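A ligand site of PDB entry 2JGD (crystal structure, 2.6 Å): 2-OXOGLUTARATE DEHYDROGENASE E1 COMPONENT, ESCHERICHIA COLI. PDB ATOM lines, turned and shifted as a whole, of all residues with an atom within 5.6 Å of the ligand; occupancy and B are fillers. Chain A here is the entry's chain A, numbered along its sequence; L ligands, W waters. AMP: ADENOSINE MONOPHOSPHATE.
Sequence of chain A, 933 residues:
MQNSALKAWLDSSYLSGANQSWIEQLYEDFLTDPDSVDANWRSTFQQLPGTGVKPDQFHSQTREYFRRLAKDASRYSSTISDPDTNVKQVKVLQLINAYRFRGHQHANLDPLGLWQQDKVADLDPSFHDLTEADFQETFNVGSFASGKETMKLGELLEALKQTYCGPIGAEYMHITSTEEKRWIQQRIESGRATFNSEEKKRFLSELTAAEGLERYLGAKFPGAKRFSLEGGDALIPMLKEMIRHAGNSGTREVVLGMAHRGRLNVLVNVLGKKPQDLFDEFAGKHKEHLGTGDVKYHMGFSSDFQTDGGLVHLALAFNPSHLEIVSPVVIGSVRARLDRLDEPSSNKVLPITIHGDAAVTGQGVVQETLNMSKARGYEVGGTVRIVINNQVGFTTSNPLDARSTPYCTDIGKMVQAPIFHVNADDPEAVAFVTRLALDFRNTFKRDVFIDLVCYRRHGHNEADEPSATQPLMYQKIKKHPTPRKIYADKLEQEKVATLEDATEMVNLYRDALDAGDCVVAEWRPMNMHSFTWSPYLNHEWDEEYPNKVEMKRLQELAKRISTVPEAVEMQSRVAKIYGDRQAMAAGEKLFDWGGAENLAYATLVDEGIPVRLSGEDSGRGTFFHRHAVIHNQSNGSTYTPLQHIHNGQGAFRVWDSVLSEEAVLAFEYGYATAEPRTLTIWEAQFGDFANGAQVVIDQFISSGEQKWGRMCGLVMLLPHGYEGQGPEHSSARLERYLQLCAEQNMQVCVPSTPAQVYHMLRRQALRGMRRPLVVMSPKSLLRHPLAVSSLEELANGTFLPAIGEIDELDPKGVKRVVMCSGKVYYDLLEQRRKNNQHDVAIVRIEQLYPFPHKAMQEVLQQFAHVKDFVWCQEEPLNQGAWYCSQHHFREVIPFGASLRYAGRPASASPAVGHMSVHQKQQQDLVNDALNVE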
ATOM      1  N   GLU A 253      -0.785  32.617  -4.735  1.00  0.00           N
ATOM      2  CA  GLU A 253      -0.477  31.180  -4.737  1.00  0.00           C
ATOM      3  C   GLU A 253      -1.724  30.274  -4.681  1.00  0.00           C
ATOM      4  O   GLU A 253      -2.758  30.621  -4.093  1.00  0.00           O
ATOM      5  CB  GLU A 253       0.463  30.835  -3.565  1.00  0.00           C
ATOM      6  CG  GLU A 253       1.795  31.597  -3.605  1.00  0.00           C
ATOM      7  CD  GLU A 253       2.545  31.554  -2.273  1.00  0.00           C
ATOM      8  OE1 GLU A 253       2.962  30.445  -1.852  1.00  0.00           O
ATOM      9  OE2 GLU A 253       2.744  32.628  -1.674  1.00  0.00           O
ATOM     10  N   PHE A 301       4.626  19.000  -7.437  1.00  0.00           N
ATOM     11  CA  PHE A 301       5.195  19.851  -8.447  1.00  0.00           C
ATOM     12  C   PHE A 301       5.001  21.278  -8.094  1.00  0.00           C
ATOM     13  O   PHE A 301       3.967  21.636  -7.526  1.00  0.00           O
ATOM     14  CB  PHE A 301       4.564  19.576  -9.795  1.00  0.00           C
ATOM     15  CG  PHE A 301       5.460  19.885 -10.936  1.00  0.00           C
ATOM     16  CD1 PHE A 301       5.369  21.092 -11.600  1.00  0.00           C
ATOM     17  CD2 PHE A 301       6.443  18.977 -11.314  1.00  0.00           C
ATOM     18  CE1 PHE A 301       6.223  21.386 -12.657  1.00  0.00           C
ATOM     19  CE2 PHE A 301       7.297  19.262 -12.377  1.00  0.00           C
ATOM     20  CZ  PHE A 301       7.175  20.470 -13.046  1.00  0.00           C
ATOM     21  N   SER A 302       5.991  22.099  -8.409  1.00  0.00           N
ATOM     22  CA  SER A 302       5.897  23.525  -8.127  1.00  0.00           C
ATOM     23  C   SER A 302       6.115  24.304  -9.405  1.00  0.00           C
ATOM     24  O   SER A 302       7.032  23.998 -10.156  1.00  0.00           O
ATOM     25  CB  SER A 302       6.956  23.919  -7.108  1.00  0.00           C
ATOM     26  OG  SER A 302       6.581  23.536  -5.791  1.00  0.00           O
ATOM     27  N   SER A 303       5.276  25.293  -9.678  1.00  0.00           N
ATOM     28  CA  SER A 303       5.556  26.182 -10.799  1.00  0.00           C
ATOM     29  C   SER A 303       4.915  27.534 -10.681  1.00  0.00           C
ATOM     30  O   SER A 303       4.132  27.812  -9.748  1.00  0.00           O
ATOM     31  CB  SER A 303       5.173  25.548 -12.123  1.00  0.00           C
ATOM     32  OG  SER A 303       3.805  25.248 -12.128  1.00  0.00           O
ATOM     33  N   HIS A 313       1.678  31.481  -8.201  1.00  0.00           N
ATOM     34  CA  HIS A 313       2.445  30.289  -7.844  1.00  0.00           C
ATOM     35  C   HIS A 313       1.527  29.090  -7.689  1.00  0.00           C
ATOM     36  O   HIS A 313       0.473  29.169  -7.039  1.00  0.00           O
ATOM     37  CB  HIS A 313       3.237  30.503  -6.555  1.00  0.00           C
ATOM     38  CG  HIS A 313       4.173  29.379  -6.239  1.00  0.00           C
ATOM     39  ND1 HIS A 313       5.186  28.985  -7.090  1.00  0.00           N
ATOM     40  CD2 HIS A 313       4.204  28.515  -5.192  1.00  0.00           C
ATOM     41  CE1 HIS A 313       5.800  27.940  -6.578  1.00  0.00           C
ATOM     42  NE2 HIS A 313       5.235  27.629  -5.424  1.00  0.00           N
ATOM     43  N   LEU A 314       1.912  27.974  -8.304  1.00  0.00           N
ATOM     44  CA  LEU A 314       1.175  26.718  -8.153  1.00  0.00           C
ATOM     45  C   LEU A 314       1.992  25.735  -7.350  1.00  0.00           C
ATOM     46  O   LEU A 314       3.193  25.550  -7.620  1.00  0.00           O
ATOM     47  CB  LEU A 314       0.860  26.100  -9.518  1.00  0.00           C
ATOM     48  CG  LEU A 314       0.106  26.990 -10.497  1.00  0.00           C
ATOM     49  CD1 LEU A 314      -0.126  26.230 -11.768  1.00  0.00           C
ATOM     50  CD2 LEU A 314      -1.205  27.402  -9.866  1.00  0.00           C
ATOM     51  N   ALA A 315       1.350  25.096  -6.375  1.00  0.00           N
ATOM     52  CA  ALA A 315       1.995  24.048  -5.596  1.00  0.00           C
ATOM     53  C   ALA A 315       1.089  22.858  -5.415  1.00  0.00           C
ATOM     54  O   ALA A 315       0.065  22.911  -4.697  1.00  0.00           O
ATOM     55  CB  ALA A 315       2.469  24.591  -4.246  1.00  0.00           C
ATOM     56  N   ARG A 337       1.700  29.881   4.408  1.00  0.00           N
ATOM     57  CA  ARG A 337       1.969  30.806   3.303  1.00  0.00           C
ATOM     58  C   ARG A 337       1.259  32.138   3.512  1.00  0.00           C
ATOM     59  O   ARG A 337       1.730  33.200   3.071  1.00  0.00           O
ATOM     60  CB  ARG A 337       1.523  30.211   1.965  1.00  0.00           C
ATOM     61  CG  ARG A 337       2.362  29.000   1.539  1.00  0.00           C
ATOM     62  CD  ARG A 337       1.759  28.296   0.317  1.00  0.00           C
ATOM     63  NE  ARG A 337       2.261  26.936   0.177  1.00  0.00           N
ATOM     64  CZ  ARG A 337       3.279  26.589  -0.591  1.00  0.00           C
ATOM     65  NH1 ARG A 337       3.908  27.509  -1.313  1.00  0.00           N
ATOM     66  NH2 ARG A 337       3.668  25.321  -0.638  1.00  0.00           N
ATOM     67  N   ARG A 340       3.062  34.440   6.081  1.00  0.00           N
ATOM     68  CA  ARG A 340       4.305  35.103   5.705  1.00  0.00           C
ATOM     69  C   ARG A 340       4.087  36.265   4.765  1.00  0.00           C
ATOM     70  O   ARG A 340       5.033  36.904   4.341  1.00  0.00           O
ATOM     71  CB  ARG A 340       5.291  34.121   5.072  1.00  0.00           C
ATOM     72  CG  ARG A 340       4.758  33.470   3.845  1.00  0.00           C
ATOM     73  CD  ARG A 340       5.851  33.019   2.941  1.00  0.00           C
ATOM     74  NE  ARG A 340       6.384  31.705   3.308  1.00  0.00           N
ATOM     75  CZ  ARG A 340       6.348  30.636   2.533  1.00  0.00           C
ATOM     76  NH1 ARG A 340       5.764  30.684   1.330  1.00  0.00           N
ATOM     77  NH2 ARG A 340       6.904  29.528   2.947  1.00  0.00           N
ATOM     78  N   MET A 526      10.200  29.270 -11.974  1.00  0.00           N
ATOM     79  CA  MET A 526      10.170  30.029 -10.744  1.00  0.00           C
ATOM     80  C   MET A 526      11.370  30.955 -10.619  1.00  0.00           C
ATOM     81  O   MET A 526      12.457  30.657 -11.105  1.00  0.00           O
ATOM     82  CB  MET A 526      10.149  29.081  -9.556  1.00  0.00           C
ATOM     83  CG  MET A 526       8.808  28.402  -9.340  1.00  0.00           C
ATOM     84  SD  MET A 526       9.017  26.933  -8.330  1.00  0.00           S
ATOM     85  CE  MET A 526       9.374  27.706  -6.767  1.00  0.00           C
ATOM     86  N   SER A 530      11.469  32.266  -4.929  1.00  0.00           N
ATOM     87  CA  SER A 530      10.461  31.227  -4.678  1.00  0.00           C
ATOM     88  C   SER A 530      11.056  29.965  -4.033  1.00  0.00           C
ATOM     89  O   SER A 530      10.306  29.084  -3.611  1.00  0.00           O
ATOM     90  CB  SER A 530       9.710  30.859  -5.957  1.00  0.00           C
ATOM     91  OG  SER A 530       8.596  31.695  -6.148  1.00  0.00           O
ATOM     92  N   PHE A 531      12.383  29.866  -3.979  1.00  0.00           N
ATOM     93  CA  PHE A 531      13.021  28.644  -3.481  1.00  0.00           C
ATOM     94  C   PHE A 531      13.378  28.811  -2.008  1.00  0.00           C
ATOM     95  O   PHE A 531      14.539  29.089  -1.642  1.00  0.00           O
ATOM     96  CB  PHE A 531      14.260  28.270  -4.303  1.00  0.00           C
ATOM     97  CG  PHE A 531      13.949  27.710  -5.670  1.00  0.00           C
ATOM     98  CD1 PHE A 531      13.813  28.560  -6.762  1.00  0.00           C
ATOM     99  CD2 PHE A 531      13.750  26.341  -5.856  1.00  0.00           C
ATOM    100  CE1 PHE A 531      13.481  28.060  -8.013  1.00  0.00           C
ATOM    101  CE2 PHE A 531      13.450  25.839  -7.102  1.00  0.00           C
ATOM    102  CZ  PHE A 531      13.314  26.698  -8.189  1.00  0.00           C
ATOM    103  N   THR A 532      12.371  28.643  -1.164  1.00  0.00           N
ATOM    104  CA  THR A 532      12.446  29.048   0.230  1.00  0.00           C
ATOM    105  C   THR A 532      13.281  28.044   1.031  1.00  0.00           C
ATOM    106  O   THR A 532      13.791  28.346   2.099  1.00  0.00           O
ATOM    107  CB  THR A 532      11.027  29.122   0.815  1.00  0.00           C
ATOM    108  OG1 THR A 532      10.252  28.044   0.289  1.00  0.00           O
ATOM    109  CG2 THR A 532      10.360  30.433   0.419  1.00  0.00           C
ATOM    110  N   TRP A 533      13.438  26.845   0.479  1.00  0.00           N
ATOM    111  CA  TRP A 533      14.106  25.758   1.169  1.00  0.00           C
ATOM    112  C   TRP A 533      15.623  25.622   0.921  1.00  0.00           C
ATOM    113  O   TRP A 533      16.312  24.917   1.670  1.00  0.00           O
ATOM    114  CB  TRP A 533      13.371  24.449   0.908  1.00  0.00           C
ATOM    115  CG  TRP A 533      12.206  24.260   1.814  1.00  0.00           C
ATOM    116  CD1 TRP A 533      10.906  24.650   1.598  1.00  0.00           C
ATOM    117  CD2 TRP A 533      12.239  23.710   3.119  1.00  0.00           C
ATOM    118  NE1 TRP A 533      10.128  24.337   2.676  1.00  0.00           N
ATOM    119  CE2 TRP A 533      10.918  23.753   3.626  1.00  0.00           C
ATOM    120  CE3 TRP A 533      13.256  23.169   3.915  1.00  0.00           C
ATOM    121  CZ2 TRP A 533      10.597  23.273   4.877  1.00  0.00           C
ATOM    122  CZ3 TRP A 533      12.923  22.676   5.165  1.00  0.00           C
ATOM    123  CH2 TRP A 533      11.611  22.740   5.637  1.00  0.00           C
ATOM    124  N   LEU A 537      18.980  22.626   2.913  1.00  0.00           N
ATOM    125  CA  LEU A 537      19.275  21.289   2.413  1.00  0.00           C
ATOM    126  C   LEU A 537      20.679  20.849   2.767  1.00  0.00           C
ATOM    127  O   LEU A 537      21.582  21.682   2.907  1.00  0.00           O
ATOM    128  CB  LEU A 537      19.080  21.231   0.907  1.00  0.00           C
ATOM    129  CG  LEU A 537      17.764  21.784   0.345  1.00  0.00           C
ATOM    130  CD1 LEU A 537      17.744  21.566  -1.127  1.00  0.00           C
ATOM    131  CD2 LEU A 537      16.551  21.129   0.994  1.00  0.00           C
ATOM    132  N   ALA A 672       4.995  23.175   8.798  1.00  0.00           N
ATOM    133  CA  ALA A 672       6.454  23.064   8.924  1.00  0.00           C
ATOM    134  C   ALA A 672       7.130  22.826   7.570  1.00  0.00           C
ATOM    135  O   ALA A 672       8.247  23.265   7.311  1.00  0.00           O
ATOM    136  CB  ALA A 672       6.802  21.910   9.881  1.00  0.00           C
ATOM    137  N   THR A 673       6.444  22.087   6.723  1.00  0.00           N
ATOM    138  CA  THR A 673       6.870  21.811   5.353  1.00  0.00           C
ATOM    139  C   THR A 673       6.905  23.016   4.421  1.00  0.00           C
ATOM    140  O   THR A 673       7.628  23.001   3.427  1.00  0.00           O
ATOM    141  CB  THR A 673       5.936  20.759   4.747  1.00  0.00           C
ATOM    142  OG1 THR A 673       6.017  19.572   5.536  1.00  0.00           O
ATOM    143  CG2 THR A 673       6.257  20.477   3.336  1.00  0.00           C
ATOM    144  N   ALA A 674       6.092  24.025   4.700  1.00  0.00           N
ATOM    145  CA  ALA A 674       6.016  25.159   3.803  1.00  0.00           C
ATOM    146  C   ALA A 674       6.940  26.260   4.262  1.00  0.00           C
ATOM    147  O   ALA A 674       7.400  27.066   3.463  1.00  0.00           O
ATOM    148  CB  ALA A 674       4.619  25.662   3.702  1.00  0.00           C
ATOM    149  N   GLY A 709      11.914  13.934  -1.154  1.00  0.00           N
ATOM    150  CA  GLY A 709      12.865  15.046  -1.013  1.00  0.00           C
ATOM    151  C   GLY A 709      12.354  16.158  -0.082  1.00  0.00           C
ATOM    152  O   GLY A 709      12.880  17.272  -0.064  1.00  0.00           O
ATOM    153  N   ARG A 710      11.349  15.845   0.714  1.00  0.00           N
ATOM    154  CA  ARG A 710      10.640  16.874   1.450  1.00  0.00           C
ATOM    155  C   ARG A 710      11.194  16.971   2.881  1.00  0.00           C
ATOM    156  O   ARG A 710      11.078  16.035   3.677  1.00  0.00           O
ATOM    157  CB  ARG A 710       9.146  16.576   1.450  1.00  0.00           C
ATOM    158  CG  ARG A 710       8.438  17.059   0.160  1.00  0.00           C
ATOM    159  CD  ARG A 710       8.499  18.557   0.170  1.00  0.00           C
ATOM    160  NE  ARG A 710       8.069  19.241  -1.042  1.00  0.00           N
ATOM    161  CZ  ARG A 710       6.950  19.931  -1.100  1.00  0.00           C
ATOM    162  NH1 ARG A 710       6.148  19.955  -0.029  1.00  0.00           N
ATOM    163  NH2 ARG A 710       6.598  20.581  -2.206  1.00  0.00           N
ATOM    164  N   MET A 711      11.849  18.093   3.178  1.00  0.00           N
ATOM    165  CA  MET A 711      12.365  18.352   4.525  1.00  0.00           C
ATOM    166  C   MET A 711      11.247  18.856   5.434  1.00  0.00           C
ATOM    167  O   MET A 711      10.221  19.346   4.968  1.00  0.00           O
ATOM    168  CB  MET A 711      13.491  19.375   4.494  1.00  0.00           C
ATOM    169  CG  MET A 711      14.648  18.998   3.607  1.00  0.00           C
ATOM    170  SD  MET A 711      15.117  17.267   3.630  1.00  0.00           S
ATOM    171  CE  MET A 711      15.798  17.131   5.258  1.00  0.00           C
ATOM    172  N   CYS A 712      11.463  18.769   6.733  1.00  0.00           N
ATOM    173  CA  CYS A 712      10.460  19.163   7.683  1.00  0.00           C
ATOM    174  C   CYS A 712      11.097  19.225   9.063  1.00  0.00           C
ATOM    175  O   CYS A 712      11.653  18.217   9.523  1.00  0.00           O
ATOM    176  CB  CYS A 712       9.335  18.125   7.680  1.00  0.00           C
ATOM    177  SG  CYS A 712       8.096  18.305   8.963  1.00  0.00           S
HETATM  178  P   AMP L   1       6.428  25.569  -2.970  1.00  0.00           P
HETATM  179  O1P AMP L   1       5.873  24.589  -1.977  1.00  0.00           O
HETATM  180  O2P AMP L   1       6.413  26.993  -2.498  1.00  0.00           O
HETATM  181  O3P AMP L   1       5.917  25.376  -4.392  1.00  0.00           O
HETATM  182  O5' AMP L   1       7.985  25.164  -3.067  1.00  0.00           O
HETATM  183  C5' AMP L   1       8.955  26.036  -3.652  1.00  0.00           C
HETATM  184  C4' AMP L   1      10.204  25.262  -4.079  1.00  0.00           C
HETATM  185  O4' AMP L   1      10.887  24.729  -2.927  1.00  0.00           O
HETATM  186  C3' AMP L   1       9.852  24.051  -4.919  1.00  0.00           C
HETATM  187  O3' AMP L   1      10.999  23.703  -5.675  1.00  0.00           O
HETATM  188  C2' AMP L   1       9.722  22.944  -3.906  1.00  0.00           C
HETATM  189  O2' AMP L   1      10.070  21.700  -4.502  1.00  0.00           O
HETATM  190  C1' AMP L   1      10.777  23.308  -2.894  1.00  0.00           C
HETATM  191  N9  AMP L   1      10.242  22.898  -1.584  1.00  0.00           N
HETATM  192  C8  AMP L   1       9.066  23.295  -1.078  1.00  0.00           C
HETATM  193  N7  AMP L   1       8.842  22.750   0.154  1.00  0.00           N
HETATM  194  C5  AMP L   1       9.903  21.956   0.429  1.00  0.00           C
HETATM  195  C6  AMP L   1      10.285  21.077   1.533  1.00  0.00           C
HETATM  196  N6  AMP L   1       9.470  20.957   2.614  1.00  0.00           N
HETATM  197  N1  AMP L   1      11.448  20.411   1.435  1.00  0.00           N
HETATM  198  C2  AMP L   1      12.246  20.535   0.346  1.00  0.00           C
HETATM  199  N3  AMP L   1      11.958  21.342  -0.706  1.00  0.00           N
HETATM  200  C4  AMP L   1      10.811  22.041  -0.722  1.00  0.00           C
HETATM  201  O   HOH W   1      10.478  22.649  -8.191  1.00  0.00           O
HETATM  202  O   HOH W   2      10.777  18.660  -2.999  1.00  0.00           O
HETATM  203  O   HOH W   3       7.150  29.472  -3.472  1.00  0.00           O
HETATM  204  O   HOH W   4      13.503  25.624  -2.114  1.00  0.00           O
HETATM  205  O   HOH W   5       6.308  24.024   0.597  1.00  0.00           O
HETATM  206  O   HOH W   6       7.402  27.354   0.405  1.00  0.00           O
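The guanidinium group of Arg 337 lies within salt-bridge range of an oxygen (O1P) of the ligand (2.7 Å).
The side-chain hydroxyl (OG) of Ser 302 sits at hydrogen-bond distance from an oxygen (O3P) of the ligand (2.4 Å).
The indole nitrogen (NE1) of Trp 533 lies close to a nitrogen (N7) of the ligand (3.2 Å).
An oxygen (O3P) of the ligand is in hydrogen-bond range of a ring nitrogen (NE2) of His 313, 2.6 Å away.
A nitrogen (N6) of the ligand sits at hydrogen-bond distance from the backbone carbonyl oxygen (O) of Thr 673 (2.9 Å).
A nitrogen (N1) of the ligand lies within hydrogen-bond range of the backbone NH (N) of Met 711 (2.9 Å).
O of Met 711 lies within hydrogen-bond range of N6 of the ligand (2.9 Å).
Water W5 lies within hydrogen-bond range of an oxygen (O1P) of the ligand (2.7 Å), the guanidinium group of Arg 337 (3.2 Å) and the backbone carbonyl oxygen of Thr 673 (3.3 Å).
Water W3 lies within hydrogen-bond range of an oxygen (O2P) of the ligand, the backbone carbonyl oxygen of Ser 530 and a ring nitrogen (NE2) of His 313.
Water W4 lies within hydrogen-bond range of the backbone NH (N) of Trp 533 (2.9 Å), an oxygen (O4') of the ligand (2.9 Å) and the backbone NH (N) of Thr 532 (3.4 Å).
Water W6 lies within hydrogen-bond range of the side-chain hydroxyl of Thr 532 (2.9 Å), the backbone carbonyl oxygen of Ala 674 (3.1 Å), an oxygen (O2P) of the ligand (3.1 Å) and the guanidinium group of Arg 340 (3.4 Å).
Water W2 bridges the guanidinium group of Arg 710 (3.4 Å) and an oxygen (O2') of the ligand (3.5 Å).
Residues that only touch the ligand: Ala 315, Met 526, Ser 530, Phe 531, Gly 709 and Arg 710.
Hydrophobic or aromatic side chains within 4 Å of the ligand: His 313, Ala 315, Met 526, Phe 531, Trp 533 and Met 711.
Within 4 Å of the ligand: Ser 302, His 313, Ala 315, Arg 337, Met 526, Ser 530, Phe 531, Trp 533, Thr 673, Gly 709, Arg 710 and Met 711.
The nearest printed residue that does not touch the ligand is Leu 314 (4.2 Å).
ND1 of His 313 is in hydrogen-bond range of O of Ser 303.
The guanidinium group (NH1) of Arg 337 lies within salt-bridge range of the side-chain carboxylate (OE1) of Glu 253 (3.1 Å).
The backbone carbonyl oxygen of Thr 673 lies within hydrogen-bond range of the indole nitrogen of Trp 533 (2.9 Å).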
